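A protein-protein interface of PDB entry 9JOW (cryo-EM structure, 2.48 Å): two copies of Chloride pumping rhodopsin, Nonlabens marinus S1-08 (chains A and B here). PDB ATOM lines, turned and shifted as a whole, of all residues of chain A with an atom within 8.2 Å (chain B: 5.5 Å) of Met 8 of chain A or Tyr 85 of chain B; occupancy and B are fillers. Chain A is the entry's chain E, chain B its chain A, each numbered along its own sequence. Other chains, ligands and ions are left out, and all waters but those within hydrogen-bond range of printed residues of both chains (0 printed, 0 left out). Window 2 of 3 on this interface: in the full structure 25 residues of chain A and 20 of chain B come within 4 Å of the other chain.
CB of Ala 19 of chain B touches O of Gly 7 of chain A (3.9 Å).
Met 8 of chain A touches Tyr 85 of chain B.
Asp 94 of chain A touches Ala 84 of chain B (O to CA, 3.7 Å).
OH of Tyr 90 of chain B touches C of Leu 95 of chain A, at 3.9 Å.
Thr 96 of chain A touches Tyr 85 of chain B (CG2 to CD2, 3.8 Å).
N of Tyr 90 of chain B lies within hydrogen-bond range of O of Tyr 17 of chain B, 2.9 Å away.
The backbone carbonyl oxygen of Ala 84 of chain B sits at hydrogen-bond distance from the backbone NH of Gln 91 of chain B (2.9 Å).
The side-chain hydroxyl (OH) of Tyr 85 of chain B lies close to the backbone carbonyl oxygen (O) of Gly 88 of chain B.
Met 8 of chain A touches one residue of chain B.
Tyr 85 of chain B touches just these residues of chain A: Met 8, Asp 94 and Thr 96.
Of chain A, only Asp 94 comes within 4 Å of Ala 84 of chain B.
Printed residues of chain B within 4 Å of Asp 94 of chain A: Ala 84 (3.7 Å) and Tyr 85 (2.9 Å).
Of the printed residues of chain A, Ala 19 of chain B touches Gly 7.
Leu 151 of chain A touches none of the printed residues of chain B.
The nearest printed residue of chain A that does not touch Ala 19 of chain B is Lys 9 of chain A (4.6 Å).
O of Asp 94 of chain A is in hydrogen-bond range of N of Tyr 85 of chain B, at 2.9 Å.
OG1 of Thr 96 of chain A is in hydrogen-bond range of OH of Tyr 90 of chain B, 2.6 Å away.
Hydrophobic or aromatic side chains of chain B that line the printed part of chain A: Ala 19, Ala 84, Tyr 85 and Tyr 90.
Of the 22 printed residues of chain A, 5 touch a printed residue of chain B.
Printed residues of chain A that touch a printed residue of chain B: Gly 7, Met 8, Asp 94, Leu 95 and Thr 96.
Along chain A the printed residues that touch a printed residue of chain B span positions 7 to 96.
Among the printed residues, 7 pairs touch across the chains.
Among the printed residues, no Asp or Glu carboxylate lies within 4 Å of a Lys or Arg side-chain nitrogen of the other chain.
Position printed for both chains: 83.
Of the 7 pairs that touch across the chains among the printed residues, none has its exchanged pair printed and touching as well.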
ATOM      1  N   GLY A   7     -16.367  -7.859  30.235  1.00  0.00           N
ATOM      2  CA  GLY A   7     -17.292  -7.768  29.087  1.00  0.00           C
ATOM      3  C   GLY A   7     -16.946  -8.772  27.985  1.00  0.00           C
ATOM      4  O   GLY A   7     -17.785  -9.560  27.586  1.00  0.00           O
ATOM      5  N   MET A   8     -15.691  -8.742  27.523  1.00  0.00           N
ATOM      6  CA  MET A   8     -15.206  -9.521  26.402  1.00  0.00           C
ATOM      7  C   MET A   8     -15.069 -11.005  26.732  1.00  0.00           C
ATOM      8  O   MET A   8     -14.814 -11.368  27.875  1.00  0.00           O
ATOM      9  CB  MET A   8     -13.816  -9.040  25.985  1.00  0.00           C
ATOM     10  CG  MET A   8     -13.790  -7.594  25.620  1.00  0.00           C
ATOM     11  SD  MET A   8     -15.104  -7.254  24.437  1.00  0.00           S
ATOM     12  CE  MET A   8     -14.527  -5.584  24.117  1.00  0.00           C
ATOM     13  N   LYS A   9     -15.189 -11.840  25.691  1.00  0.00           N
ATOM     14  CA  LYS A   9     -14.999 -13.270  25.841  1.00  0.00           C
ATOM     15  C   LYS A   9     -13.613 -13.734  25.378  1.00  0.00           C
ATOM     16  O   LYS A   9     -13.095 -14.719  25.887  1.00  0.00           O
ATOM     17  CB  LYS A   9     -16.056 -14.092  25.117  1.00  0.00           C
ATOM     18  CG  LYS A   9     -17.447 -13.582  25.217  1.00  0.00           C
ATOM     19  CD  LYS A   9     -17.873 -13.405  26.652  1.00  0.00           C
ATOM     20  CE  LYS A   9     -18.410 -14.640  27.188  1.00  0.00           C
ATOM     21  NZ  LYS A   9     -18.714 -14.347  28.599  1.00  0.00           N
ATOM     22  N   ASN A  10     -13.010 -13.054  24.419  1.00  0.00           N
ATOM     23  CA  ASN A  10     -11.778 -13.545  23.840  1.00  0.00           C
ATOM     24  C   ASN A  10     -10.695 -12.496  24.039  1.00  0.00           C
ATOM     25  O   ASN A  10     -10.959 -11.306  24.028  1.00  0.00           O
ATOM     26  CB  ASN A  10     -11.982 -13.900  22.367  1.00  0.00           C
ATOM     27  CG  ASN A  10     -12.587 -15.266  22.101  1.00  0.00           C
ATOM     28  OD1 ASN A  10     -12.795 -15.616  20.931  1.00  0.00           O
ATOM     29  ND2 ASN A  10     -12.885 -16.062  23.126  1.00  0.00           N
ATOM     30  N   ILE A  11      -9.462 -12.946  24.184  1.00  0.00           N
ATOM     31  CA  ILE A  11      -8.380 -12.028  24.448  1.00  0.00           C
ATOM     32  C   ILE A  11      -7.984 -11.241  23.200  1.00  0.00           C
ATOM     33  O   ILE A  11      -7.391 -10.169  23.333  1.00  0.00           O
ATOM     34  CB  ILE A  11      -7.182 -12.763  25.046  1.00  0.00           C
ATOM     35  CG1 ILE A  11      -6.575 -13.744  24.075  1.00  0.00           C
ATOM     36  CG2 ILE A  11      -7.576 -13.434  26.350  1.00  0.00           C
ATOM     37  CD1 ILE A  11      -5.225 -14.262  24.557  1.00  0.00           C
ATOM     38  N   GLU A  12      -8.299 -11.711  21.999  1.00  0.00           N
ATOM     39  CA  GLU A  12      -8.079 -10.869  20.821  1.00  0.00           C
ATOM     40  C   GLU A  12      -8.583  -9.449  21.086  1.00  0.00           C
ATOM     41  O   GLU A  12      -7.876  -8.491  20.818  1.00  0.00           O
ATOM     42  CB  GLU A  12      -8.752 -11.396  19.565  1.00  0.00           C
ATOM     43  CG  GLU A  12      -8.044 -12.610  18.966  1.00  0.00           C
ATOM     44  CD  GLU A  12      -8.058 -13.954  19.706  1.00  0.00           C
ATOM     45  OE1 GLU A  12      -8.704 -14.081  20.773  1.00  0.00           O
ATOM     46  OE2 GLU A  12      -7.393 -14.902  19.203  1.00  0.00           O
ATOM     47  N   SER A  13      -9.744  -9.330  21.731  1.00  0.00           N
ATOM     48  CA  SER A  13     -10.407  -8.049  21.925  1.00  0.00           C
ATOM     49  C   SER A  13      -9.822  -7.243  23.081  1.00  0.00           C
ATOM     50  O   SER A  13     -10.177  -6.077  23.243  1.00  0.00           O
ATOM     51  CB  SER A  13     -11.909  -8.219  22.095  1.00  0.00           C
ATOM     52  OG  SER A  13     -12.557  -8.287  20.837  1.00  0.00           O
ATOM     53  N   LEU A  14      -8.862  -7.786  23.830  1.00  0.00           N
ATOM     54  CA  LEU A  14      -8.275  -7.031  24.924  1.00  0.00           C
ATOM     55  C   LEU A  14      -7.098  -6.146  24.512  1.00  0.00           C
ATOM     56  O   LEU A  14      -6.766  -5.220  25.252  1.00  0.00           O
ATOM     57  CB  LEU A  14      -7.807  -7.957  26.019  1.00  0.00           C
ATOM     58  CG  LEU A  14      -8.874  -8.821  26.673  1.00  0.00           C
ATOM     59  CD1 LEU A  14      -8.147  -9.709  27.690  1.00  0.00           C
ATOM     60  CD2 LEU A  14      -9.880  -7.953  27.294  1.00  0.00           C
ATOM     61  N   PHE A  15      -6.441  -6.415  23.384  1.00  0.00           N
ATOM     62  CA  PHE A  15      -5.178  -5.747  23.101  1.00  0.00           C
ATOM     63  C   PHE A  15      -5.251  -4.747  21.951  1.00  0.00           C
ATOM     64  O   PHE A  15      -6.239  -4.671  21.214  1.00  0.00           O
ATOM     65  CB  PHE A  15      -4.131  -6.803  22.776  1.00  0.00           C
ATOM     66  CG  PHE A  15      -4.085  -7.851  23.868  1.00  0.00           C
ATOM     67  CD1 PHE A  15      -3.897  -7.485  25.192  1.00  0.00           C
ATOM     68  CD2 PHE A  15      -4.280  -9.196  23.568  1.00  0.00           C
ATOM     69  CE1 PHE A  15      -3.855  -8.451  26.180  1.00  0.00           C
ATOM     70  CE2 PHE A  15      -4.233 -10.156  24.566  1.00  0.00           C
ATOM     71  CZ  PHE A  15      -4.047  -9.785  25.867  1.00  0.00           C
ATOM     72  N   TYR A  83     -11.040  -3.298  14.019  1.00  0.00           N
ATOM     73  CA  TYR A  83      -9.949  -2.436  14.448  1.00  0.00           C
ATOM     74  C   TYR A  83      -9.686  -1.281  13.492  1.00  0.00           C
ATOM     75  O   TYR A  83      -9.930  -1.394  12.298  1.00  0.00           O
ATOM     76  CB  TYR A  83      -8.621  -3.130  14.682  1.00  0.00           C
ATOM     77  CG  TYR A  83      -8.737  -4.210  15.728  1.00  0.00           C
ATOM     78  CD1 TYR A  83      -9.346  -5.421  15.404  1.00  0.00           C
ATOM     79  CD2 TYR A  83      -8.246  -4.030  17.015  1.00  0.00           C
ATOM     80  CE1 TYR A  83      -9.434  -6.443  16.332  1.00  0.00           C
ATOM     81  CE2 TYR A  83      -8.387  -5.031  17.975  1.00  0.00           C
ATOM     82  CZ  TYR A  83      -8.943  -6.248  17.616  1.00  0.00           C
ATOM     83  OH  TYR A  83      -9.103  -7.264  18.514  1.00  0.00           O
ATOM     84  N   LEU A  92      -9.373  -1.565  19.048  1.00  0.00           N
ATOM     85  CA  LEU A  92     -10.739  -2.010  18.857  1.00  0.00           C
ATOM     86  C   LEU A  92     -11.684  -0.824  18.717  1.00  0.00           C
ATOM     87  O   LEU A  92     -11.487   0.190  19.399  1.00  0.00           O
ATOM     88  CB  LEU A  92     -11.174  -2.825  20.055  1.00  0.00           C
ATOM     89  CG  LEU A  92     -12.326  -3.795  19.803  1.00  0.00           C
ATOM     90  CD1 LEU A  92     -11.953  -4.884  18.824  1.00  0.00           C
ATOM     91  CD2 LEU A  92     -12.789  -4.421  21.085  1.00  0.00           C
ATOM     92  N   GLN A  93     -12.766  -1.039  17.939  1.00  0.00           N
ATOM     93  CA  GLN A  93     -13.741  -0.018  17.578  1.00  0.00           C
ATOM     94  C   GLN A  93     -15.160  -0.555  17.378  1.00  0.00           C
ATOM     95  O   GLN A  93     -15.504  -0.949  16.260  1.00  0.00           O
ATOM     96  CB  GLN A  93     -13.489   0.319  16.108  1.00  0.00           C
ATOM     97  CG  GLN A  93     -12.085   0.676  15.710  1.00  0.00           C
ATOM     98  CD  GLN A  93     -11.811   2.097  16.077  1.00  0.00           C
ATOM     99  OE1 GLN A  93     -12.498   2.990  15.570  1.00  0.00           O
ATOM    100  NE2 GLN A  93     -10.822   2.296  16.944  1.00  0.00           N
ATOM    101  N   ASP A  94     -16.017  -0.619  18.373  1.00  0.00           N
ATOM    102  CA  ASP A  94     -17.464  -0.783  18.085  1.00  0.00           C
ATOM    103  C   ASP A  94     -17.942  -2.148  17.548  1.00  0.00           C
ATOM    104  O   ASP A  94     -19.131  -2.344  17.359  1.00  0.00           O
ATOM    105  CB  ASP A  94     -17.997   0.263  17.125  1.00  0.00           C
ATOM    106  CG  ASP A  94     -18.088  -0.141  15.661  1.00  0.00           C
ATOM    107  OD1 ASP A  94     -17.047  -0.142  14.953  1.00  0.00           O
ATOM    108  OD2 ASP A  94     -19.216  -0.479  15.247  1.00  0.00           O
ATOM    109  N   LEU A  95     -17.037  -3.080  17.292  1.00  0.00           N
ATOM    110  CA  LEU A  95     -17.345  -4.479  17.094  1.00  0.00           C
ATOM    111  C   LEU A  95     -16.321  -5.268  17.890  1.00  0.00           C
ATOM    112  O   LEU A  95     -15.356  -4.697  18.354  1.00  0.00           O
ATOM    113  CB  LEU A  95     -17.175  -4.665  15.604  1.00  0.00           C
ATOM    114  CG  LEU A  95     -18.123  -5.609  14.890  1.00  0.00           C
ATOM    115  CD1 LEU A  95     -19.531  -5.113  15.029  1.00  0.00           C
ATOM    116  CD2 LEU A  95     -17.651  -5.662  13.434  1.00  0.00           C
ATOM    117  N   THR A  96     -16.552  -6.558  18.100  1.00  0.00           N
ATOM    118  CA  THR A  96     -15.607  -7.387  18.840  1.00  0.00           C
ATOM    119  C   THR A  96     -15.206  -8.544  17.934  1.00  0.00           C
ATOM    120  O   THR A  96     -15.941  -8.933  17.033  1.00  0.00           O
ATOM    121  CB  THR A  96     -16.208  -7.866  20.168  1.00  0.00           C
ATOM    122  OG1 THR A  96     -17.395  -8.630  19.957  1.00  0.00           O
ATOM    123  CG2 THR A  96     -16.655  -6.737  21.080  1.00  0.00           C
ATOM    124  N   PHE A  97     -14.021  -9.069  18.158  1.00  0.00           N
ATOM    125  CA  PHE A  97     -13.503 -10.149  17.349  1.00  0.00           C
ATOM    126  C   PHE A  97     -13.511 -11.385  18.241  1.00  0.00           C
ATOM    127  O   PHE A  97     -13.231 -11.278  19.437  1.00  0.00           O
ATOM    128  CB  PHE A  97     -12.138  -9.690  16.811  1.00  0.00           C
ATOM    129  CG  PHE A  97     -11.544 -10.724  15.881  1.00  0.00           C
ATOM    130  CD1 PHE A  97     -11.838 -10.684  14.517  1.00  0.00           C
ATOM    131  CD2 PHE A  97     -10.830 -11.805  16.374  1.00  0.00           C
ATOM    132  CE1 PHE A  97     -11.404 -11.682  13.672  1.00  0.00           C
ATOM    133  CE2 PHE A  97     -10.346 -12.774  15.499  1.00  0.00           C
ATOM    134  CZ  PHE A  97     -10.649 -12.709  14.157  1.00  0.00           C
ATOM    135  N   GLN A 150     -14.089 -21.957  26.099  1.00  0.00           N
ATOM    136  CA  GLN A 150     -13.311 -20.808  25.641  1.00  0.00           C
ATOM    137  C   GLN A 150     -14.097 -19.522  25.848  1.00  0.00           C
ATOM    138  O   GLN A 150     -13.606 -18.440  25.502  1.00  0.00           O
ATOM    139  CB  GLN A 150     -12.738 -20.900  24.226  1.00  0.00           C
ATOM    140  CG  GLN A 150     -13.793 -21.128  23.151  1.00  0.00           C
ATOM    141  CD  GLN A 150     -14.495 -19.892  22.648  1.00  0.00           C
ATOM    142  OE1 GLN A 150     -13.872 -19.019  22.035  1.00  0.00           O
ATOM    143  NE2 GLN A 150     -15.813 -19.859  22.832  1.00  0.00           N
ATOM    144  N   LEU A 151     -15.291 -19.654  26.428  1.00  0.00           N
ATOM    145  CA  LEU A 151     -16.004 -18.528  27.009  1.00  0.00           C
ATOM    146  C   LEU A 151     -15.345 -18.032  28.283  1.00  0.00           C
ATOM    147  O   LEU A 151     -15.586 -16.884  28.649  1.00  0.00           O
ATOM    148  CB  LEU A 151     -17.477 -18.874  27.252  1.00  0.00           C
ATOM    149  CG  LEU A 151     -18.239 -19.107  25.941  1.00  0.00           C
ATOM    150  CD1 LEU A 151     -19.661 -19.423  26.193  1.00  0.00           C
ATOM    151  CD2 LEU A 151     -18.092 -17.929  25.018  1.00  0.00           C
ATOM    152  N   TYR A 152     -14.440 -18.815  28.899  1.00  0.00           N
ATOM    153  CA  TYR A 152     -13.811 -18.343  30.129  1.00  0.00           C
ATOM    154  C   TYR A 152     -12.386 -17.841  29.916  1.00  0.00           C
ATOM    155  O   TYR A 152     -11.650 -17.660  30.875  1.00  0.00           O
ATOM    156  CB  TYR A 152     -13.845 -19.469  31.146  1.00  0.00           C
ATOM    157  CG  TYR A 152     -15.263 -19.813  31.518  1.00  0.00           C
ATOM    158  CD1 TYR A 152     -15.924 -19.081  32.471  1.00  0.00           C
ATOM    159  CD2 TYR A 152     -15.941 -20.861  30.917  1.00  0.00           C
ATOM    160  CE1 TYR A 152     -17.212 -19.416  32.866  1.00  0.00           C
ATOM    161  CE2 TYR A 152     -17.241 -21.182  31.266  1.00  0.00           C
ATOM    162  CZ  TYR A 152     -17.880 -20.451  32.247  1.00  0.00           C
ATOM    163  OH  TYR A 152     -19.166 -20.705  32.619  1.00  0.00           O
ATOM    164  N   GLU A 153     -11.976 -17.542  28.690  1.00  0.00           N
ATOM    165  CA  GLU A 153     -10.553 -17.312  28.496  1.00  0.00           C
ATOM    166  C   GLU A 153     -10.101 -15.947  29.035  1.00  0.00           C
ATOM    167  O   GLU A 153      -8.912 -15.765  29.288  1.00  0.00           O
ATOM    168  CB  GLU A 153     -10.177 -17.618  27.051  1.00  0.00           C
ATOM    169  CG  GLU A 153     -10.408 -16.493  26.058  1.00  0.00           C
ATOM    170  CD  GLU A 153      -9.851 -16.873  24.685  1.00  0.00           C
ATOM    171  OE1 GLU A 153      -9.944 -18.073  24.312  1.00  0.00           O
ATOM    172  OE2 GLU A 153      -9.334 -15.980  23.976  1.00  0.00           O
ATOM    173  N   VAL A 154     -11.027 -15.005  29.242  1.00  0.00           N
ATOM    174  CA  VAL A 154     -10.703 -13.705  29.814  1.00  0.00           C
ATOM    175  C   VAL A 154     -11.065 -13.669  31.299  1.00  0.00           C
ATOM    176  O   VAL A 154     -10.314 -13.146  32.111  1.00  0.00           O
ATOM    177  CB  VAL A 154     -11.421 -12.591  29.041  1.00  0.00           C
ATOM    178  CG1 VAL A 154     -11.299 -11.274  29.782  1.00  0.00           C
ATOM    179  CG2 VAL A 154     -10.920 -12.460  27.599  1.00  0.00           C
ATOM    180  N   ASP A 155     -12.189 -14.296  31.652  1.00  0.00           N
ATOM    181  CA  ASP A 155     -12.672 -14.322  33.025  1.00  0.00           C
ATOM    182  C   ASP A 155     -11.912 -15.341  33.872  1.00  0.00           C
ATOM    183  O   ASP A 155     -11.188 -14.953  34.791  1.00  0.00           O
ATOM    184  CB  ASP A 155     -14.156 -14.637  33.098  1.00  0.00           C
ATOM    185  CG  ASP A 155     -15.095 -13.619  32.469  1.00  0.00           C
ATOM    186  OD1 ASP A 155     -14.604 -12.611  31.910  1.00  0.00           O
ATOM    187  OD2 ASP A 155     -16.319 -13.847  32.541  1.00  0.00           O
ATOM    188  N   TYR B  17     -27.633  -6.738  23.909  1.00  0.00           N
ATOM    189  CA  TYR B  17     -27.080  -8.071  24.021  1.00  0.00           C
ATOM    190  C   TYR B  17     -25.693  -7.935  24.620  1.00  0.00           C
ATOM    191  O   TYR B  17     -24.968  -7.012  24.278  1.00  0.00           O
ATOM    192  CB  TYR B  17     -27.043  -8.750  22.637  1.00  0.00           C
ATOM    193  CG  TYR B  17     -28.432  -8.855  22.042  1.00  0.00           C
ATOM    194  CD1 TYR B  17     -29.279  -9.905  22.378  1.00  0.00           C
ATOM    195  CD2 TYR B  17     -28.894  -7.902  21.158  1.00  0.00           C
ATOM    196  CE1 TYR B  17     -30.555 -10.003  21.843  1.00  0.00           C
ATOM    197  CE2 TYR B  17     -30.166  -7.978  20.625  1.00  0.00           C
ATOM    198  CZ  TYR B  17     -31.001  -9.019  20.989  1.00  0.00           C
ATOM    199  OH  TYR B  17     -32.270  -9.104  20.492  1.00  0.00           O
ATOM    200  N   SER B  18     -25.343  -8.859  25.519  1.00  0.00           N
ATOM    201  CA  SER B  18     -23.965  -9.047  25.923  1.00  0.00           C
ATOM    202  C   SER B  18     -23.128  -9.464  24.722  1.00  0.00           C
ATOM    203  O   SER B  18     -23.656 -10.100  23.809  1.00  0.00           O
ATOM    204  CB  SER B  18     -23.898 -10.077  26.970  1.00  0.00           C
ATOM    205  OG  SER B  18     -24.377 -11.342  26.533  1.00  0.00           O
ATOM    206  N   ALA B  19     -21.815  -9.209  24.804  1.00  0.00           N
ATOM    207  CA  ALA B  19     -20.880  -9.675  23.796  1.00  0.00           C
ATOM    208  C   ALA B  19     -21.003 -11.181  23.539  1.00  0.00           C
ATOM    209  O   ALA B  19     -20.972 -11.628  22.395  1.00  0.00           O
ATOM    210  CB  ALA B  19     -19.495  -9.292  24.142  1.00  0.00           C
ATOM    211  N   TYR B  83     -26.351  -3.663  14.788  1.00  0.00           N
ATOM    212  CA  TYR B  83     -25.911  -3.398  16.158  1.00  0.00           C
ATOM    213  C   TYR B  83     -24.464  -2.933  16.248  1.00  0.00           C
ATOM    214  O   TYR B  83     -23.644  -3.287  15.401  1.00  0.00           O
ATOM    215  CB  TYR B  83     -26.044  -4.570  17.124  1.00  0.00           C
ATOM    216  CG  TYR B  83     -27.481  -5.026  17.241  1.00  0.00           C
ATOM    217  CD1 TYR B  83     -28.043  -5.776  16.219  1.00  0.00           C
ATOM    218  CD2 TYR B  83     -28.260  -4.708  18.350  1.00  0.00           C
ATOM    219  CE1 TYR B  83     -29.330  -6.274  16.317  1.00  0.00           C
ATOM    220  CE2 TYR B  83     -29.586  -5.127  18.422  1.00  0.00           C
ATOM    221  CZ  TYR B  83     -30.106  -5.935  17.413  1.00  0.00           C
ATOM    222  OH  TYR B  83     -31.387  -6.390  17.447  1.00  0.00           O
ATOM    223  N   ALA B  84     -24.165  -2.180  17.324  1.00  0.00           N
ATOM    224  CA  ALA B  84     -22.793  -1.778  17.605  1.00  0.00           C
ATOM    225  C   ALA B  84     -22.472  -1.976  19.063  1.00  0.00           C
ATOM    226  O   ALA B  84     -23.359  -1.876  19.888  1.00  0.00           O
ATOM    227  CB  ALA B  84     -22.582  -0.344  17.308  1.00  0.00           C
ATOM    228  N   TYR B  85     -21.197  -2.237  19.354  1.00  0.00           N
ATOM    229  CA  TYR B  85     -20.780  -2.403  20.730  1.00  0.00           C
ATOM    230  C   TYR B  85     -20.532  -1.020  21.331  1.00  0.00           C
ATOM    231  O   TYR B  85     -19.722  -0.259  20.806  1.00  0.00           O
ATOM    232  CB  TYR B  85     -19.541  -3.293  20.813  1.00  0.00           C
ATOM    233  CG  TYR B  85     -19.288  -3.832  22.220  1.00  0.00           C
ATOM    234  CD1 TYR B  85     -20.269  -4.538  22.911  1.00  0.00           C
ATOM    235  CD2 TYR B  85     -18.067  -3.647  22.859  1.00  0.00           C
ATOM    236  CE1 TYR B  85     -20.041  -5.053  24.173  1.00  0.00           C
ATOM    237  CE2 TYR B  85     -17.833  -4.140  24.136  1.00  0.00           C
ATOM    238  CZ  TYR B  85     -18.828  -4.844  24.796  1.00  0.00           C
ATOM    239  OH  TYR B  85     -18.653  -5.385  26.046  1.00  0.00           O
ATOM    240  N   VAL B  86     -21.227  -0.715  22.428  1.00  0.00           N
ATOM    241  CA  VAL B  86     -21.264   0.641  22.967  1.00  0.00           C
ATOM    242  C   VAL B  86     -21.598   0.619  24.442  1.00  0.00           C
ATOM    243  O   VAL B  86     -22.699   0.209  24.794  1.00  0.00           O
ATOM    244  CB  VAL B  86     -22.340   1.489  22.289  1.00  0.00           C
ATOM    245  CG1 VAL B  86     -22.134   2.925  22.704  1.00  0.00           C
ATOM    246  CG2 VAL B  86     -22.305   1.308  20.772  1.00  0.00           C
ATOM    247  N   ASP B  87     -20.663   1.051  25.294  1.00  0.00           N
ATOM    248  CA  ASP B  87     -20.854   0.983  26.742  1.00  0.00           C
ATOM    249  C   ASP B  87     -21.092  -0.467  27.167  1.00  0.00           C
ATOM    250  O   ASP B  87     -22.071  -0.780  27.856  1.00  0.00           O
ATOM    251  CB  ASP B  87     -21.949   1.933  27.206  1.00  0.00           C
ATOM    252  CG  ASP B  87     -21.927   3.304  26.540  1.00  0.00           C
ATOM    253  OD1 ASP B  87     -20.830   3.902  26.453  1.00  0.00           O
ATOM    254  OD2 ASP B  87     -23.010   3.765  26.109  1.00  0.00           O
ATOM    255  N   GLY B  88     -20.218  -1.358  26.673  1.00  0.00           N
ATOM    256  CA  GLY B  88     -20.181  -2.745  27.108  1.00  0.00           C
ATOM    257  C   GLY B  88     -21.433  -3.572  26.783  1.00  0.00           C
ATOM    258  O   GLY B  88     -21.698  -4.571  27.448  1.00  0.00           O
ATOM    259  N   SER B  89     -22.201  -3.158  25.766  1.00  0.00           N
ATOM    260  CA  SER B  89     -23.284  -3.964  25.242  1.00  0.00           C
ATOM    261  C   SER B  89     -23.463  -3.646  23.774  1.00  0.00           C
ATOM    262  O   SER B  89     -23.110  -2.568  23.311  1.00  0.00           O
ATOM    263  CB  SER B  89     -24.585  -3.768  25.952  1.00  0.00           C
ATOM    264  OG  SER B  89     -25.116  -2.499  25.618  1.00  0.00           O
ATOM    265  N   TYR B  90     -23.999  -4.620  23.055  1.00  0.00           N
ATOM    266  CA  TYR B  90     -24.410  -4.378  21.693  1.00  0.00           C
ATOM    267  C   TYR B  90     -25.773  -3.714  21.746  1.00  0.00           C
ATOM    268  O   TYR B  90     -26.697  -4.274  22.348  1.00  0.00           O
ATOM    269  CB  TYR B  90     -24.445  -5.730  20.972  1.00  0.00           C
ATOM    270  CG  TYR B  90     -23.094  -6.167  20.472  1.00  0.00           C
ATOM    271  CD1 TYR B  90     -22.637  -5.723  19.251  1.00  0.00           C
ATOM    272  CD2 TYR B  90     -22.275  -6.998  21.222  1.00  0.00           C
ATOM    273  CE1 TYR B  90     -21.388  -6.084  18.771  1.00  0.00           C
ATOM    274  CE2 TYR B  90     -21.030  -7.387  20.746  1.00  0.00           C
ATOM    275  CZ  TYR B  90     -20.588  -6.936  19.510  1.00  0.00           C
ATOM    276  OH  TYR B  90     -19.386  -7.335  19.003  1.00  0.00           O
ATOM    277  N   GLN B  91     -25.935  -2.621  21.003  1.00  0.00           N
ATOM    278  CA  GLN B  91     -27.183  -1.877  20.955  1.00  0.00           C
ATOM    279  C   GLN B  91     -27.589  -1.555  19.523  1.00  0.00           C
ATOM    280  O   GLN B  91     -26.744  -1.289  18.668  1.00  0.00           O
ATOM    281  CB  GLN B  91     -26.871  -0.583  21.668  1.00  0.00           C
ATOM    282  CG  GLN B  91     -26.507  -0.778  23.130  1.00  0.00           C
ATOM    283  CD  GLN B  91     -26.373   0.529  23.874  1.00  0.00           C
ATOM    284  OE1 GLN B  91     -27.328   1.297  24.012  1.00  0.00           O
ATOM    285  NE2 GLN B  91     -25.172   0.803  24.345  1.00  0.00           N
